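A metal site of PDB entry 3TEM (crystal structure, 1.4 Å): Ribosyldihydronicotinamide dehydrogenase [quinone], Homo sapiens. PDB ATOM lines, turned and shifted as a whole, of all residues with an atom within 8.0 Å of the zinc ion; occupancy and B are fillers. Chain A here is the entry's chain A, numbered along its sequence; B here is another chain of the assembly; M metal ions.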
ATOM      1  N   TYR A 131     -25.082  24.806  16.908  1.00  0.00           N
ATOM      2  CA  TYR A 131     -25.749  24.054  15.852  1.00  0.00           C
ATOM      3  C   TYR A 131     -24.934  24.178  14.559  1.00  0.00           C
ATOM      4  O   TYR A 131     -23.761  23.850  14.563  1.00  0.00           O
ATOM      5  CB  TYR A 131     -27.241  24.444  15.764  1.00  0.00           C
ATOM      6  CG  TYR A 131     -28.066  23.909  16.939  1.00  0.00           C
ATOM      7  CD1 TYR A 131     -28.042  22.546  17.289  1.00  0.00           C
ATOM      8  CD2 TYR A 131     -28.782  24.760  17.776  1.00  0.00           C
ATOM      9  CE1 TYR A 131     -28.782  22.062  18.346  1.00  0.00           C
ATOM     10  CE2 TYR A 131     -29.521  24.269  18.873  1.00  0.00           C
ATOM     11  CZ  TYR A 131     -29.508  22.921  19.174  1.00  0.00           C
ATOM     12  OH  TYR A 131     -30.211  22.397  20.231  1.00  0.00           O
ATOM     13  N   ASP A 132     -25.513  24.635  13.454  1.00  0.00           N
ATOM     14  CA  ASP A 132     -24.782  24.585  12.199  1.00  0.00           C
ATOM     15  C   ASP A 132     -23.512  25.453  12.240  1.00  0.00           C
ATOM     16  O   ASP A 132     -22.561  25.186  11.510  1.00  0.00           O
ATOM     17  CB  ASP A 132     -25.689  25.004  11.031  1.00  0.00           C
ATOM     18  CG  ASP A 132     -26.794  23.982  10.748  1.00  0.00           C
ATOM     19  OD1 ASP A 132     -26.675  22.821  11.199  1.00  0.00           O
ATOM     20  OD2 ASP A 132     -27.769  24.346  10.054  1.00  0.00           O
ATOM     21  N   TRP A 168     -32.092  11.852  20.662  1.00  0.00           N
ATOM     22  CA  TRP A 168     -32.200  13.311  20.553  1.00  0.00           C
ATOM     23  C   TRP A 168     -31.195  14.111  21.422  1.00  0.00           C
ATOM     24  O   TRP A 168     -30.531  15.005  20.904  1.00  0.00           O
ATOM     25  CB  TRP A 168     -33.630  13.704  20.863  1.00  0.00           C
ATOM     26  CG  TRP A 168     -33.940  15.156  20.939  1.00  0.00           C
ATOM     27  CD1 TRP A 168     -34.255  15.879  22.051  1.00  0.00           C
ATOM     28  CD2 TRP A 168     -34.064  16.043  19.839  1.00  0.00           C
ATOM     29  NE1 TRP A 168     -34.526  17.165  21.722  1.00  0.00           N
ATOM     30  CE2 TRP A 168     -34.452  17.300  20.357  1.00  0.00           C
ATOM     31  CE3 TRP A 168     -33.896  15.913  18.452  1.00  0.00           C
ATOM     32  CZ2 TRP A 168     -34.638  18.420  19.552  1.00  0.00           C
ATOM     33  CZ3 TRP A 168     -34.113  17.028  17.640  1.00  0.00           C
ATOM     34  CH2 TRP A 168     -34.490  18.261  18.209  1.00  0.00           C
ATOM     35  N   LEU A 170     -28.328  13.299  22.561  1.00  0.00           N
ATOM     36  CA  LEU A 170     -26.961  12.996  22.154  1.00  0.00           C
ATOM     37  C   LEU A 170     -26.678  13.570  20.754  1.00  0.00           C
ATOM     38  O   LEU A 170     -25.721  14.339  20.546  1.00  0.00           O
ATOM     39  CB  LEU A 170     -26.742  11.492  22.167  1.00  0.00           C
ATOM     40  CG  LEU A 170     -27.016  10.833  23.534  1.00  0.00           C
ATOM     41  CD1 LEU A 170     -27.034   9.300  23.358  1.00  0.00           C
ATOM     42  CD2 LEU A 170     -25.970  11.294  24.516  1.00  0.00           C
ATOM     43  N   GLN A 171     -27.492  13.207  19.786  1.00  0.00           N
ATOM     44  CA  GLN A 171     -27.244  13.639  18.413  1.00  0.00           C
ATOM     45  C   GLN A 171     -27.491  15.122  18.222  1.00  0.00           C
ATOM     46  O   GLN A 171     -26.688  15.774  17.581  1.00  0.00           O
ATOM     47  CB  GLN A 171     -28.107  12.840  17.418  1.00  0.00           C
ATOM     48  CG  GLN A 171     -27.664  11.387  17.401  1.00  0.00           C
ATOM     49  CD  GLN A 171     -28.322  10.527  16.306  1.00  0.00           C
ATOM     50  OE1 GLN A 171     -27.730   9.543  15.859  1.00  0.00           O
ATOM     51  NE2 GLN A 171     -29.507  10.895  15.863  1.00  0.00           N
ATOM     52  N   HIS A 172     -28.606  15.591  18.713  1.00  0.00           N
ATOM     53  CA  HIS A 172     -29.019  16.961  18.510  1.00  0.00           C
ATOM     54  C   HIS A 172     -28.519  17.894  19.609  1.00  0.00           C
ATOM     55  O   HIS A 172     -27.833  18.870  19.324  1.00  0.00           O
ATOM     56  CB  HIS A 172     -30.534  17.085  18.391  1.00  0.00           C
ATOM     57  CG  HIS A 172     -30.979  18.472  18.058  1.00  0.00           C
ATOM     58  ND1 HIS A 172     -30.781  19.039  16.813  1.00  0.00           N
ATOM     59  CD2 HIS A 172     -31.581  19.415  18.826  1.00  0.00           C
ATOM     60  CE1 HIS A 172     -31.279  20.265  16.829  1.00  0.00           C
ATOM     61  NE2 HIS A 172     -31.735  20.522  18.035  1.00  0.00           N
ATOM     62  N   GLY A 173     -28.839  17.589  20.843  1.00  0.00           N
ATOM     63  CA  GLY A 173     -28.531  18.479  21.955  1.00  0.00           C
ATOM     64  C   GLY A 173     -27.041  18.614  22.185  1.00  0.00           C
ATOM     65  O   GLY A 173     -26.597  19.661  22.668  1.00  0.00           O
ATOM     66  N   THR A 174     -26.277  17.593  21.773  1.00  0.00           N
ATOM     67  CA  THR A 174     -24.848  17.587  22.011  1.00  0.00           C
ATOM     68  C   THR A 174     -24.078  17.715  20.709  1.00  0.00           C
ATOM     69  O   THR A 174     -23.418  18.716  20.474  1.00  0.00           O
ATOM     70  CB  THR A 174     -24.422  16.317  22.816  1.00  0.00           C
ATOM     71  OG1 THR A 174     -25.230  16.176  23.993  1.00  0.00           O
ATOM     72  CG2 THR A 174     -22.947  16.441  23.266  1.00  0.00           C
ATOM     73  N   LEU A 175     -24.128  16.709  19.880  1.00  0.00           N
ATOM     74  CA  LEU A 175     -23.251  16.689  18.709  1.00  0.00           C
ATOM     75  C   LEU A 175     -23.572  17.778  17.689  1.00  0.00           C
ATOM     76  O   LEU A 175     -22.691  18.512  17.272  1.00  0.00           O
ATOM     77  CB  LEU A 175     -23.250  15.288  18.079  1.00  0.00           C
ATOM     78  CG  LEU A 175     -22.744  14.209  19.053  1.00  0.00           C
ATOM     79  CD1 LEU A 175     -23.033  12.847  18.418  1.00  0.00           C
ATOM     80  CD2 LEU A 175     -21.285  14.352  19.347  1.00  0.00           C
ATOM     81  N   HIS A 176     -24.831  17.881  17.294  1.00  0.00           N
ATOM     82  CA  HIS A 176     -25.210  18.903  16.339  1.00  0.00           C
ATOM     83  C   HIS A 176     -24.955  20.267  16.988  1.00  0.00           C
ATOM     84  O   HIS A 176     -24.520  21.176  16.287  1.00  0.00           O
ATOM     85  CB  HIS A 176     -26.690  18.710  15.968  1.00  0.00           C
ATOM     86  CG  HIS A 176     -27.186  19.593  14.879  1.00  0.00           C
ATOM     87  ND1 HIS A 176     -28.511  19.581  14.505  1.00  0.00           N
ATOM     88  CD2 HIS A 176     -26.582  20.539  14.125  1.00  0.00           C
ATOM     89  CE1 HIS A 176     -28.691  20.474  13.529  1.00  0.00           C
ATOM     90  NE2 HIS A 176     -27.537  21.067  13.285  1.00  0.00           N
ATOM     91  N   PHE A 177     -25.235  20.417  18.274  1.00  0.00           N
ATOM     92  CA  PHE A 177     -25.041  21.707  18.938  1.00  0.00           C
ATOM     93  C   PHE A 177     -23.602  22.181  18.745  1.00  0.00           C
ATOM     94  O   PHE A 177     -23.340  23.365  18.550  1.00  0.00           O
ATOM     95  CB  PHE A 177     -25.412  21.638  20.411  1.00  0.00           C
ATOM     96  CG  PHE A 177     -25.376  22.970  21.112  1.00  0.00           C
ATOM     97  CD1 PHE A 177     -26.498  23.780  21.111  1.00  0.00           C
ATOM     98  CD2 PHE A 177     -24.254  23.405  21.815  1.00  0.00           C
ATOM     99  CE1 PHE A 177     -26.494  25.015  21.753  1.00  0.00           C
ATOM    100  CE2 PHE A 177     -24.247  24.636  22.474  1.00  0.00           C
ATOM    101  CZ  PHE A 177     -25.358  25.418  22.449  1.00  0.00           C
ATOM    102  N   PHE A 180     -21.102  19.242  14.773  1.00  0.00           N
ATOM    103  CA  PHE A 180     -20.888  18.000  14.061  1.00  0.00           C
ATOM    104  C   PHE A 180     -22.013  17.760  13.061  1.00  0.00           C
ATOM    105  O   PHE A 180     -23.187  18.079  13.312  1.00  0.00           O
ATOM    106  CB  PHE A 180     -20.932  16.805  15.012  1.00  0.00           C
ATOM    107  CG  PHE A 180     -19.691  16.591  15.831  1.00  0.00           C
ATOM    108  CD1 PHE A 180     -19.668  16.954  17.176  1.00  0.00           C
ATOM    109  CD2 PHE A 180     -18.587  15.950  15.304  1.00  0.00           C
ATOM    110  CE1 PHE A 180     -18.547  16.701  17.971  1.00  0.00           C
ATOM    111  CE2 PHE A 180     -17.474  15.693  16.094  1.00  0.00           C
ATOM    112  CZ  PHE A 180     -17.456  16.048  17.412  1.00  0.00           C
ATOM    113  N   VAL A 182     -23.932  14.477  11.774  1.00  0.00           N
ATOM    114  CA  VAL A 182     -24.158  13.225  12.444  1.00  0.00           C
ATOM    115  C   VAL A 182     -24.449  12.151  11.409  1.00  0.00           C
ATOM    116  O   VAL A 182     -25.406  12.265  10.633  1.00  0.00           O
ATOM    117  CB  VAL A 182     -25.338  13.403  13.402  1.00  0.00           C
ATOM    118  CG1 VAL A 182     -25.718  12.056  14.050  1.00  0.00           C
ATOM    119  CG2 VAL A 182     -24.965  14.459  14.488  1.00  0.00           C
ATOM    120  N   ILE A 219     -27.250  12.454   8.511  1.00  0.00           N
ATOM    121  CA  ILE A 219     -28.697  12.558   8.599  1.00  0.00           C
ATOM    122  C   ILE A 219     -29.099  14.018   8.720  1.00  0.00           C
ATOM    123  O   ILE A 219     -28.298  14.878   9.096  1.00  0.00           O
ATOM    124  CB  ILE A 219     -29.237  11.873   9.858  1.00  0.00           C
ATOM    125  CG1 ILE A 219     -28.719  12.553  11.143  1.00  0.00           C
ATOM    126  CG2 ILE A 219     -28.881  10.409   9.831  1.00  0.00           C
ATOM    127  CD1 ILE A 219     -29.353  12.033  12.413  1.00  0.00           C
ATOM    128  N   PRO A 220     -30.368  14.318   8.439  1.00  0.00           N
ATOM    129  CA  PRO A 220     -30.902  15.626   8.798  1.00  0.00           C
ATOM    130  C   PRO A 220     -31.231  15.590  10.267  1.00  0.00           C
ATOM    131  O   PRO A 220     -32.198  14.959  10.695  1.00  0.00           O
ATOM    132  CB  PRO A 220     -32.158  15.749   7.930  1.00  0.00           C
ATOM    133  CG  PRO A 220     -32.565  14.317   7.647  1.00  0.00           C
ATOM    134  CD  PRO A 220     -31.319  13.480   7.695  1.00  0.00           C
ATOM    135  N   CYS A 221     -30.392  16.200  11.082  1.00  0.00           N
ATOM    136  CA  CYS A 221     -30.517  16.076  12.521  1.00  0.00           C
ATOM    137  C   CYS A 221     -31.527  17.081  13.039  1.00  0.00           C
ATOM    138  O   CYS A 221     -31.185  18.114  13.629  1.00  0.00           O
ATOM    139  CB  CYS A 221     -29.148  16.272  13.178  1.00  0.00           C
ATOM    140  SG  CYS A 221     -29.178  16.026  14.986  1.00  0.00           S
ATOM    141  N   THR A 222     -32.789  16.775  12.781  1.00  0.00           N
ATOM    142  CA  THR A 222     -33.887  17.653  13.132  1.00  0.00           C
ATOM    143  C   THR A 222     -34.903  16.959  14.010  1.00  0.00           C
ATOM    144  O   THR A 222     -34.887  15.747  14.148  1.00  0.00           O
ATOM    145  CB  THR A 222     -34.594  18.060  11.847  1.00  0.00           C
ATOM    146  OG1 THR A 222     -35.196  16.896  11.245  1.00  0.00           O
ATOM    147  CG2 THR A 222     -33.596  18.689  10.873  1.00  0.00           C
ATOM    148  N   ALA A 223     -35.825  17.730  14.594  1.00  0.00           N
ATOM    149  CA  ALA A 223     -36.922  17.137  15.322  1.00  0.00           C
ATOM    150  C   ALA A 223     -37.729  16.193  14.421  1.00  0.00           C
ATOM    151  O   ALA A 223     -38.141  15.133  14.890  1.00  0.00           O
ATOM    152  CB  ALA A 223     -37.861  18.227  15.918  1.00  0.00           C
ATOM    153  N   TRP A 225     -36.724  14.272  11.929  1.00  0.00           N
ATOM    154  CA  TRP A 225     -36.047  12.988  11.794  1.00  0.00           C
ATOM    155  C   TRP A 225     -36.210  12.153  13.050  1.00  0.00           C
ATOM    156  O   TRP A 225     -36.491  10.956  12.994  1.00  0.00           O
ATOM    157  CB  TRP A 225     -34.563  13.214  11.513  1.00  0.00           C
ATOM    158  CG  TRP A 225     -33.802  11.956  11.215  1.00  0.00           C
ATOM    159  CD1 TRP A 225     -33.589  11.399   9.994  1.00  0.00           C
ATOM    160  CD2 TRP A 225     -33.143  11.096  12.175  1.00  0.00           C
ATOM    161  NE1 TRP A 225     -32.793  10.285  10.111  1.00  0.00           N
ATOM    162  CE2 TRP A 225     -32.542  10.046  11.437  1.00  0.00           C
ATOM    163  CE3 TRP A 225     -33.005  11.093  13.567  1.00  0.00           C
ATOM    164  CZ2 TRP A 225     -31.792   9.039  12.035  1.00  0.00           C
ATOM    165  CZ3 TRP A 225     -32.247  10.079  14.174  1.00  0.00           C
ATOM    166  CH2 TRP A 225     -31.669   9.052  13.386  1.00  0.00           C
ATOM    167  N   HIS A 226     -36.096  12.792  14.219  1.00  0.00           N
ATOM    168  CA  HIS A 226     -36.182  12.035  15.472  1.00  0.00           C
ATOM    169  C   HIS A 226     -37.587  11.596  15.883  1.00  0.00           C
ATOM    170  O   HIS A 226     -37.753  10.522  16.470  1.00  0.00           O
ATOM    171  CB  HIS A 226     -35.550  12.845  16.613  1.00  0.00           C
ATOM    172  CG  HIS A 226     -34.064  12.944  16.521  1.00  0.00           C
ATOM    173  ND1 HIS A 226     -33.411  13.859  15.723  1.00  0.00           N
ATOM    174  CD2 HIS A 226     -33.096  12.232  17.156  1.00  0.00           C
ATOM    175  CE1 HIS A 226     -32.099  13.707  15.867  1.00  0.00           C
ATOM    176  NE2 HIS A 226     -31.882  12.735  16.728  1.00  0.00           N
ATOM    177  N   VAL B 159     -35.104  26.081  18.298  1.00  0.00           N
ATOM    178  CA  VAL B 159     -33.856  25.386  17.953  1.00  0.00           C
ATOM    179  C   VAL B 159     -33.584  24.133  18.782  1.00  0.00           C
ATOM    180  O   VAL B 159     -32.938  23.200  18.284  1.00  0.00           O
ATOM    181  CB  VAL B 159     -32.616  26.318  18.031  1.00  0.00           C
ATOM    182  CG1 VAL B 159     -32.689  27.361  16.912  1.00  0.00           C
ATOM    183  CG2 VAL B 159     -32.490  26.947  19.415  1.00  0.00           C
HETATM  184 ZN    ZN M   1     -29.870  18.157  15.189  1.00  0.00          ZN
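OD1 of Asp 132 sits at hydrogen-bond distance from NE2 of His 176.
The backbone carbonyl oxygen of Gln 171 sits close to the side-chain sulfur of Cys 221, 3.6 Å away.
A ring nitrogen (NE2) of His 172 sits at hydrogen-bond distance from the side-chain hydroxyl (OH) of Tyr 131 (3.3 Å).
A ring nitrogen (NE2) of His 172 is in hydrogen-bond range of the backbone carbonyl oxygen (O) of Val 159 of chain B (2.9 Å).
O of Gln 171 is in hydrogen-bond range of N of His 176.
The backbone carbonyl oxygen (O) of His 172 lies within hydrogen-bond range of the backbone NH (N) of Phe 177 (3.2 Å).
Three residues have an atom within 4 Å of the zinc ion: His 172, His 176 and Cys 221.
The nearest printed residue that does not touch the zinc ion is Thr 222 (4.03 Å).
The zinc ion is bound by O of Cys 221 (2.0 Å), ND1 of His 172 (2.1 Å), ND1 of His 176 (2.1 Å) and SG of Cys 221 (2.2 Å).
The zinc ion has four donor atoms within binding distance.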
